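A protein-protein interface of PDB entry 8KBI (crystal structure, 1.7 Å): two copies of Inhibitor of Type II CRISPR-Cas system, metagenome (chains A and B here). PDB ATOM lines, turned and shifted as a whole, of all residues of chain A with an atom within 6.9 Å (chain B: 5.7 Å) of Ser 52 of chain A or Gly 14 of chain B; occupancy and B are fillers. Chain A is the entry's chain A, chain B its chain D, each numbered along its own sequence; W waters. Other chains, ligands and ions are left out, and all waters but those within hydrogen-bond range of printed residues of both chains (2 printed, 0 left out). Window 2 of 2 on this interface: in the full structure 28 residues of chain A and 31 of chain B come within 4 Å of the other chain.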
ATOM      1  N   LEU A  49      10.054 -21.808  15.767  1.00  0.00           N
ATOM      2  CA  LEU A  49       8.763 -22.482  15.638  1.00  0.00           C
ATOM      3  C   LEU A  49       8.909 -23.487  14.512  1.00  0.00           C
ATOM      4  O   LEU A  49       9.435 -23.175  13.474  1.00  0.00           O
ATOM      5  CB  LEU A  49       7.634 -21.547  15.337  1.00  0.00           C
ATOM      6  CG  LEU A  49       7.143 -20.576  16.394  1.00  0.00           C
ATOM      7  CD1 LEU A  49       6.113 -19.673  15.758  1.00  0.00           C
ATOM      8  CD2 LEU A  49       6.552 -21.330  17.566  1.00  0.00           C
ATOM      9  N   PRO A  50       8.463 -24.712  14.733  1.00  0.00           N
ATOM     10  CA  PRO A  50       8.569 -25.728  13.704  1.00  0.00           C
ATOM     11  C   PRO A  50       7.653 -25.486  12.500  1.00  0.00           C
ATOM     12  O   PRO A  50       6.604 -24.897  12.635  1.00  0.00           O
ATOM     13  CB  PRO A  50       8.191 -27.002  14.432  1.00  0.00           C
ATOM     14  CG  PRO A  50       7.345 -26.567  15.564  1.00  0.00           C
ATOM     15  CD  PRO A  50       7.871 -25.231  15.974  1.00  0.00           C
ATOM     16  N   GLU A  51       8.078 -25.946  11.323  1.00  0.00           N
ATOM     17  CA  GLU A  51       7.269 -25.658  10.152  1.00  0.00           C
ATOM     18  C   GLU A  51       5.854 -26.212  10.299  1.00  0.00           C
ATOM     19  O   GLU A  51       4.888 -25.566   9.890  1.00  0.00           O
ATOM     20  CB  GLU A  51       7.954 -26.187   8.891  1.00  0.00           C
ATOM     21  CG  GLU A  51       7.074 -25.969   7.681  1.00  0.00           C
ATOM     22  CD  GLU A  51       6.922 -24.495   7.376  1.00  0.00           C
ATOM     23  OE1 GLU A  51       7.874 -23.732   7.671  1.00  0.00           O
ATOM     24  OE2 GLU A  51       5.828 -24.092   6.907  1.00  0.00           O
ATOM     25  N   SER A  52       5.701 -27.393  10.908  1.00  0.00           N
ATOM     26  CA  SER A  52       4.357 -27.946  11.117  1.00  0.00           C
ATOM     27  C   SER A  52       3.471 -27.013  11.947  1.00  0.00           C
ATOM     28  O   SER A  52       2.273 -26.879  11.684  1.00  0.00           O
ATOM     29  CB  SER A  52       4.461 -29.305  11.784  1.00  0.00           C
ATOM     30  OG  SER A  52       5.140 -29.176  13.024  1.00  0.00           O
ATOM     31  N   PHE A  53       4.034 -26.344  12.954  1.00  0.00           N
ATOM     32  CA  PHE A  53       3.208 -25.415  13.722  1.00  0.00           C
ATOM     33  C   PHE A  53       2.824 -24.198  12.897  1.00  0.00           C
ATOM     34  O   PHE A  53       1.683 -23.733  12.953  1.00  0.00           O
ATOM     35  CB  PHE A  53       3.952 -24.953  14.972  1.00  0.00           C
ATOM     36  CG  PHE A  53       3.153 -24.051  15.839  1.00  0.00           C
ATOM     37  CD1 PHE A  53       2.066 -24.529  16.555  1.00  0.00           C
ATOM     38  CD2 PHE A  53       3.454 -22.715  15.908  1.00  0.00           C
ATOM     39  CE1 PHE A  53       1.319 -23.677  17.370  1.00  0.00           C
ATOM     40  CE2 PHE A  53       2.719 -21.859  16.713  1.00  0.00           C
ATOM     41  CZ  PHE A  53       1.655 -22.339  17.442  1.00  0.00           C
ATOM     42  N   LYS A  54       3.773 -23.639  12.150  1.00  0.00           N
ATOM     43  CA  LYS A  54       3.436 -22.517  11.282  1.00  0.00           C
ATOM     44  C   LYS A  54       2.375 -22.905  10.258  1.00  0.00           C
ATOM     45  O   LYS A  54       1.458 -22.123   9.981  1.00  0.00           O
ATOM     46  CB  LYS A  54       4.701 -22.002  10.608  1.00  0.00           C
ATOM     47  CG  LYS A  54       5.622 -21.382  11.614  1.00  0.00           C
ATOM     48  CD  LYS A  54       6.806 -20.714  10.998  1.00  0.00           C
ATOM     49  CE  LYS A  54       7.910 -21.722  10.879  1.00  0.00           C
ATOM     50  NZ  LYS A  54       9.253 -21.106  10.867  1.00  0.00           N
ATOM     51  N   ARG A  55       2.450 -24.127   9.727  1.00  0.00           N
ATOM     52  CA  ARG A  55       1.419 -24.595   8.804  1.00  0.00           C
ATOM     53  C   ARG A  55       0.065 -24.692   9.495  1.00  0.00           C
ATOM     54  O   ARG A  55      -0.958 -24.317   8.919  1.00  0.00           O
ATOM     55  CB  ARG A  55       1.800 -25.960   8.221  1.00  0.00           C
ATOM     56  CG  ARG A  55       2.869 -25.980   7.144  1.00  0.00           C
ATOM     57  CD  ARG A  55       2.595 -27.186   6.240  1.00  0.00           C
ATOM     58  NE  ARG A  55       2.674 -28.413   7.036  1.00  0.00           N
ATOM     59  CZ  ARG A  55       3.788 -29.048   7.408  1.00  0.00           C
ATOM     60  NH1 ARG A  55       4.989 -28.621   7.007  1.00  0.00           N
ATOM     61  NH2 ARG A  55       3.686 -30.149   8.168  1.00  0.00           N
ATOM     62  N   TRP A  56       0.031 -25.214  10.734  1.00  0.00           N
ATOM     63  CA  TRP A  56      -1.233 -25.305  11.466  1.00  0.00           C
ATOM     64  C   TRP A  56      -1.858 -23.922  11.665  1.00  0.00           C
ATOM     65  O   TRP A  56      -3.068 -23.732  11.453  1.00  0.00           O
ATOM     66  CB  TRP A  56      -1.000 -26.004  12.825  1.00  0.00           C
ATOM     67  CG  TRP A  56      -2.250 -26.140  13.634  1.00  0.00           C
ATOM     68  CD1 TRP A  56      -3.162 -27.139  13.573  1.00  0.00           C
ATOM     69  CD2 TRP A  56      -2.726 -25.220  14.611  1.00  0.00           C
ATOM     70  NE1 TRP A  56      -4.194 -26.896  14.442  1.00  0.00           N
ATOM     71  CE2 TRP A  56      -3.946 -25.720  15.096  1.00  0.00           C
ATOM     72  CE3 TRP A  56      -2.240 -24.015  15.120  1.00  0.00           C
ATOM     73  CZ2 TRP A  56      -4.685 -25.063  16.074  1.00  0.00           C
ATOM     74  CZ3 TRP A  56      -2.979 -23.361  16.103  1.00  0.00           C
ATOM     75  CH2 TRP A  56      -4.189 -23.884  16.556  1.00  0.00           C
ATOM     76  N   VAL A  57      -1.048 -22.935  12.074  1.00  0.00           N
ATOM     77  CA  VAL A  57      -1.552 -21.572  12.229  1.00  0.00           C
ATOM     78  C   VAL A  57      -2.073 -21.036  10.894  1.00  0.00           C
ATOM     79  O   VAL A  57      -3.152 -20.441  10.822  1.00  0.00           O
ATOM     80  CB  VAL A  57      -0.462 -20.654  12.811  1.00  0.00           C
ATOM     81  CG1 VAL A  57      -0.960 -19.226  12.821  1.00  0.00           C
ATOM     82  CG2 VAL A  57      -0.065 -21.110  14.235  1.00  0.00           C
ATOM     83  N   ASN A  59      -3.162 -22.642   8.224  1.00  0.00           N
ATOM     84  CA  ASN A  59      -4.370 -23.346   7.829  1.00  0.00           C
ATOM     85  C   ASN A  59      -5.549 -23.008   8.718  1.00  0.00           C
ATOM     86  O   ASN A  59      -6.686 -23.312   8.349  1.00  0.00           O
ATOM     87  CB  ASN A  59      -4.156 -24.858   7.863  1.00  0.00           C
ATOM     88  CG  ASN A  59      -3.181 -25.328   6.819  1.00  0.00           C
ATOM     89  OD1 ASN A  59      -3.148 -24.806   5.704  1.00  0.00           O
ATOM     90  ND2 ASN A  59      -2.422 -26.364   7.150  1.00  0.00           N
ATOM     91  N   GLU B   9      10.974 -38.661  19.845  1.00  0.00           N
ATOM     92  CA  GLU B   9      11.790 -38.683  18.629  1.00  0.00           C
ATOM     93  C   GLU B   9      11.049 -38.017  17.471  1.00  0.00           C
ATOM     94  O   GLU B   9      11.642 -37.285  16.657  1.00  0.00           O
ATOM     95  CB  GLU B   9      12.197 -40.121  18.311  1.00  0.00           C
ATOM     96  CG  GLU B   9      13.066 -40.727  19.405  1.00  0.00           C
ATOM     97  CD  GLU B   9      14.303 -39.882  19.664  1.00  0.00           C
ATOM     98  OE1 GLU B   9      14.615 -39.529  20.843  1.00  0.00           O
ATOM     99  OE2 GLU B   9      14.964 -39.559  18.651  1.00  0.00           O
ATOM    100  N   SER B  10       9.721 -38.173  17.438  1.00  0.00           N
ATOM    101  CA  SER B  10       8.922 -37.485  16.430  1.00  0.00           C
ATOM    102  C   SER B  10       8.922 -35.976  16.647  1.00  0.00           C
ATOM    103  O   SER B  10       9.017 -35.188  15.697  1.00  0.00           O
ATOM    104  CB  SER B  10       7.502 -38.045  16.468  1.00  0.00           C
ATOM    105  OG  SER B  10       6.713 -37.419  15.508  1.00  0.00           O
ATOM    106  N   LEU B  11       8.797 -35.562  17.904  1.00  0.00           N
ATOM    107  CA  LEU B  11       8.881 -34.145  18.248  1.00  0.00           C
ATOM    108  C   LEU B  11      10.209 -33.539  17.801  1.00  0.00           C
ATOM    109  O   LEU B  11      10.243 -32.411  17.310  1.00  0.00           O
ATOM    110  CB  LEU B  11       8.729 -33.998  19.766  1.00  0.00           C
ATOM    111  CG  LEU B  11       7.293 -34.080  20.296  1.00  0.00           C
ATOM    112  CD1 LEU B  11       7.272 -34.388  21.787  1.00  0.00           C
ATOM    113  CD2 LEU B  11       6.548 -32.767  20.007  1.00  0.00           C
ATOM    114  N   LYS B  12      11.302 -34.246  18.043  1.00  0.00           N
ATOM    115  CA  LYS B  12      12.615 -33.715  17.678  1.00  0.00           C
ATOM    116  C   LYS B  12      12.723 -33.556  16.179  1.00  0.00           C
ATOM    117  O   LYS B  12      13.543 -32.761  15.701  1.00  0.00           O
ATOM    118  CB  LYS B  12      13.721 -34.635  18.161  1.00  0.00           C
ATOM    119  CG  LYS B  12      13.822 -34.750  19.670  1.00  0.00           C
ATOM    120  CD  LYS B  12      14.795 -35.811  20.030  1.00  0.00           C
ATOM    121  CE  LYS B  12      14.923 -35.954  21.523  1.00  0.00           C
ATOM    122  NZ  LYS B  12      15.807 -37.100  21.839  1.00  0.00           N
ATOM    123  N   ARG B  13      11.946 -34.328  15.426  1.00  0.00           N
ATOM    124  CA  ARG B  13      11.994 -34.199  13.975  1.00  0.00           C
ATOM    125  C   ARG B  13      10.891 -33.289  13.429  1.00  0.00           C
ATOM    126  O   ARG B  13      10.513 -33.413  12.251  1.00  0.00           O
ATOM    127  CB  ARG B  13      11.977 -35.581  13.331  1.00  0.00           C
ATOM    128  CG  ARG B  13      13.305 -36.284  13.517  1.00  0.00           C
ATOM    129  CD  ARG B  13      13.242 -37.829  13.421  1.00  0.00           C
ATOM    130  NE  ARG B  13      14.562 -38.421  13.704  1.00  0.00           N
ATOM    131  CZ  ARG B  13      15.092 -38.566  14.927  1.00  0.00           C
ATOM    132  NH1 ARG B  13      14.415 -38.219  16.020  1.00  0.00           N
ATOM    133  NH2 ARG B  13      16.296 -39.100  15.073  1.00  0.00           N
ATOM    134  N   GLY B  14      10.353 -32.392  14.268  1.00  0.00           N
ATOM    135  CA  GLY B  14       9.469 -31.301  13.870  1.00  0.00           C
ATOM    136  C   GLY B  14       7.980 -31.597  13.777  1.00  0.00           C
ATOM    137  O   GLY B  14       7.234 -30.775  13.211  1.00  0.00           O
ATOM    138  N   HIS B  15       7.523 -32.712  14.326  1.00  0.00           N
ATOM    139  CA  HIS B  15       6.127 -33.129  14.265  1.00  0.00           C
ATOM    140  C   HIS B  15       5.311 -32.556  15.435  1.00  0.00           C
ATOM    141  O   HIS B  15       5.855 -32.184  16.477  1.00  0.00           O
ATOM    142  CB  HIS B  15       6.046 -34.653  14.279  1.00  0.00           C
ATOM    143  CG  HIS B  15       6.587 -35.290  13.031  1.00  0.00           C
ATOM    144  ND1 HIS B  15       5.859 -35.371  11.863  1.00  0.00           N
ATOM    145  CD2 HIS B  15       7.795 -35.837  12.765  1.00  0.00           C
ATOM    146  CE1 HIS B  15       6.590 -35.961  10.933  1.00  0.00           C
ATOM    147  NE2 HIS B  15       7.771 -36.249  11.451  1.00  0.00           N
ATOM    148  N   LEU B  16       3.992 -32.467  15.226  1.00  0.00           N
ATOM    149  CA  LEU B  16       3.028 -32.204  16.294  1.00  0.00           C
ATOM    150  C   LEU B  16       2.499 -33.555  16.760  1.00  0.00           C
ATOM    151  O   LEU B  16       2.081 -34.368  15.924  1.00  0.00           O
ATOM    152  CB  LEU B  16       1.860 -31.344  15.804  1.00  0.00           C
ATOM    153  CG  LEU B  16       2.197 -30.150  14.896  1.00  0.00           C
ATOM    154  CD1 LEU B  16       0.950 -29.360  14.511  1.00  0.00           C
ATOM    155  CD2 LEU B  16       3.218 -29.231  15.615  1.00  0.00           C
ATOM    156  N   PHE B  30       4.544 -29.558  20.685  1.00  0.00           N
ATOM    157  CA  PHE B  30       5.536 -29.416  19.626  1.00  0.00           C
ATOM    158  C   PHE B  30       6.850 -28.978  20.260  1.00  0.00           C
ATOM    159  O   PHE B  30       6.874 -28.527  21.404  1.00  0.00           O
ATOM    160  CB  PHE B  30       5.087 -28.430  18.537  1.00  0.00           C
ATOM    161  CG  PHE B  30       4.764 -27.018  19.026  1.00  0.00           C
ATOM    162  CD1 PHE B  30       3.501 -26.700  19.509  1.00  0.00           C
ATOM    163  CD2 PHE B  30       5.716 -25.981  18.928  1.00  0.00           C
ATOM    164  CE1 PHE B  30       3.199 -25.394  19.960  1.00  0.00           C
ATOM    165  CE2 PHE B  30       5.411 -24.663  19.331  1.00  0.00           C
ATOM    166  CZ  PHE B  30       4.167 -24.358  19.854  1.00  0.00           C
ATOM    167  N   GLU B 104       0.537 -34.061  13.187  1.00  0.00           N
ATOM    168  CA  GLU B 104       0.979 -33.609  11.850  1.00  0.00           C
ATOM    169  C   GLU B 104       2.466 -33.896  11.743  1.00  0.00           C
ATOM    170  O   GLU B 104       3.187 -33.712  12.726  1.00  0.00           O
ATOM    171  CB  GLU B 104       0.717 -32.120  11.602  1.00  0.00           C
ATOM    172  CG  GLU B 104      -0.755 -31.685  11.599  1.00  0.00           C
ATOM    173  CD  GLU B 104      -0.998 -30.240  11.106  1.00  0.00           C
ATOM    174  OE1 GLU B 104      -2.130 -29.731  11.313  1.00  0.00           O
ATOM    175  OE2 GLU B 104      -0.106 -29.652  10.444  1.00  0.00           O
ATOM    176  OXT GLU B 104       2.997 -34.314  10.707  1.00  0.00           O
HETATM  177  O   HOH W   1       7.951 -29.230  11.205  1.00  0.00           O
HETATM  178  O   HOH W   2       4.598 -32.615   9.433  1.00  0.00           O
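The backbone carbonyl oxygen (O) of Gly 14 of chain B sits at hydrogen-bond distance from the side-chain hydroxyl (OG) of Ser 52 of chain A (2.6 Å).
A ring nitrogen (ND1) of His 15 of chain B sits at hydrogen-bond distance from the chain-end carboxylate of Glu 104 of chain B (3.3 Å).
NZ of Lys 54 of chain A lies within hydrogen-bond range of O of Leu 49 of chain A (3.3 Å).
The chain-end carboxylate (O) of Glu 104 of chain B is in hydrogen-bond range of the backbone NH (N) of Leu 16 of chain B.
Among the printed residues, pairs that only touch across the chains: Leu 49 of chain A with Phe 30 of chain B (3.9 Å), Pro 50 of chain A with Phe 30 of chain B (3.7 Å), Ser 52 of chain A with Leu 16 of chain B (3.2 Å), Ser 52 of chain A with Glu 104 of chain B (3.9 Å), Phe 53 of chain A with Phe 30 of chain B (3.6 Å) and Trp 56 of chain A with Glu 104 of chain B (3.6 Å).
Of chain B, only Gly 14 (2.6 Å), Leu 16 (3.2 Å) and Glu 104 (3.9 Å) come within 4 Å of Ser 52 of chain A.
Of chain A, only Ser 52 comes within 4 Å of Gly 14 of chain B.
Printed residues of chain B within 4 Å of Leu 49 of chain A: Phe 30.
Of the printed residues of chain A, Phe 30 of chain B touches Leu 49 (3.9 Å), Pro 50 (3.7 Å) and Phe 53 (3.6 Å).
Of the printed residues of chain B, Phe 53 of chain A touches Phe 30.
Printed residues of chain B within 4 Å of Trp 56 of chain A: Glu 104 (3.6 Å).
Printed residues of chain B within 4 Å of Pro 50 of chain A: Phe 30.
Arg 13 of chain B touches none of the printed residues of chain A.
The nearest residue of chain A that does not touch Gly 14 of chain B is Pro 50 of chain A (4.1 Å).
The nearest printed residue of chain B that does not touch Phe 53 of chain A is Leu 16 of chain B (4.01 Å).
Of the 10 printed residues of chain B, 4 touch a printed residue of chain A.
Hydrophobic or aromatic side chains of chain B within 4 Å of the printed part of chain A: Leu 16 and Phe 30.
Printed residues of chain A that touch a printed residue of chain B: Leu 49, Pro 50, Ser 52, Phe 53 and Trp 56.
Hydrophobic or aromatic side chains of chain A that line the printed part of chain B: Leu 49, Pro 50, Phe 53 and Trp 56.
Among the printed residues, no Asp or Glu carboxylate lies within 4 Å of a Lys or Arg side-chain nitrogen of the other chain.
No position is printed for both chains.
Water W1 lies within hydrogen-bond range of the backbone carbonyl oxygen of Gly 14 of chain B, the backbone NH of Ser 52 of chain A and the backbone NH of Glu 51 of chain A.
Water W2 lies within hydrogen-bond range of OXT of Glu 104 of chain B and NH2 of Arg 55 of chain A.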
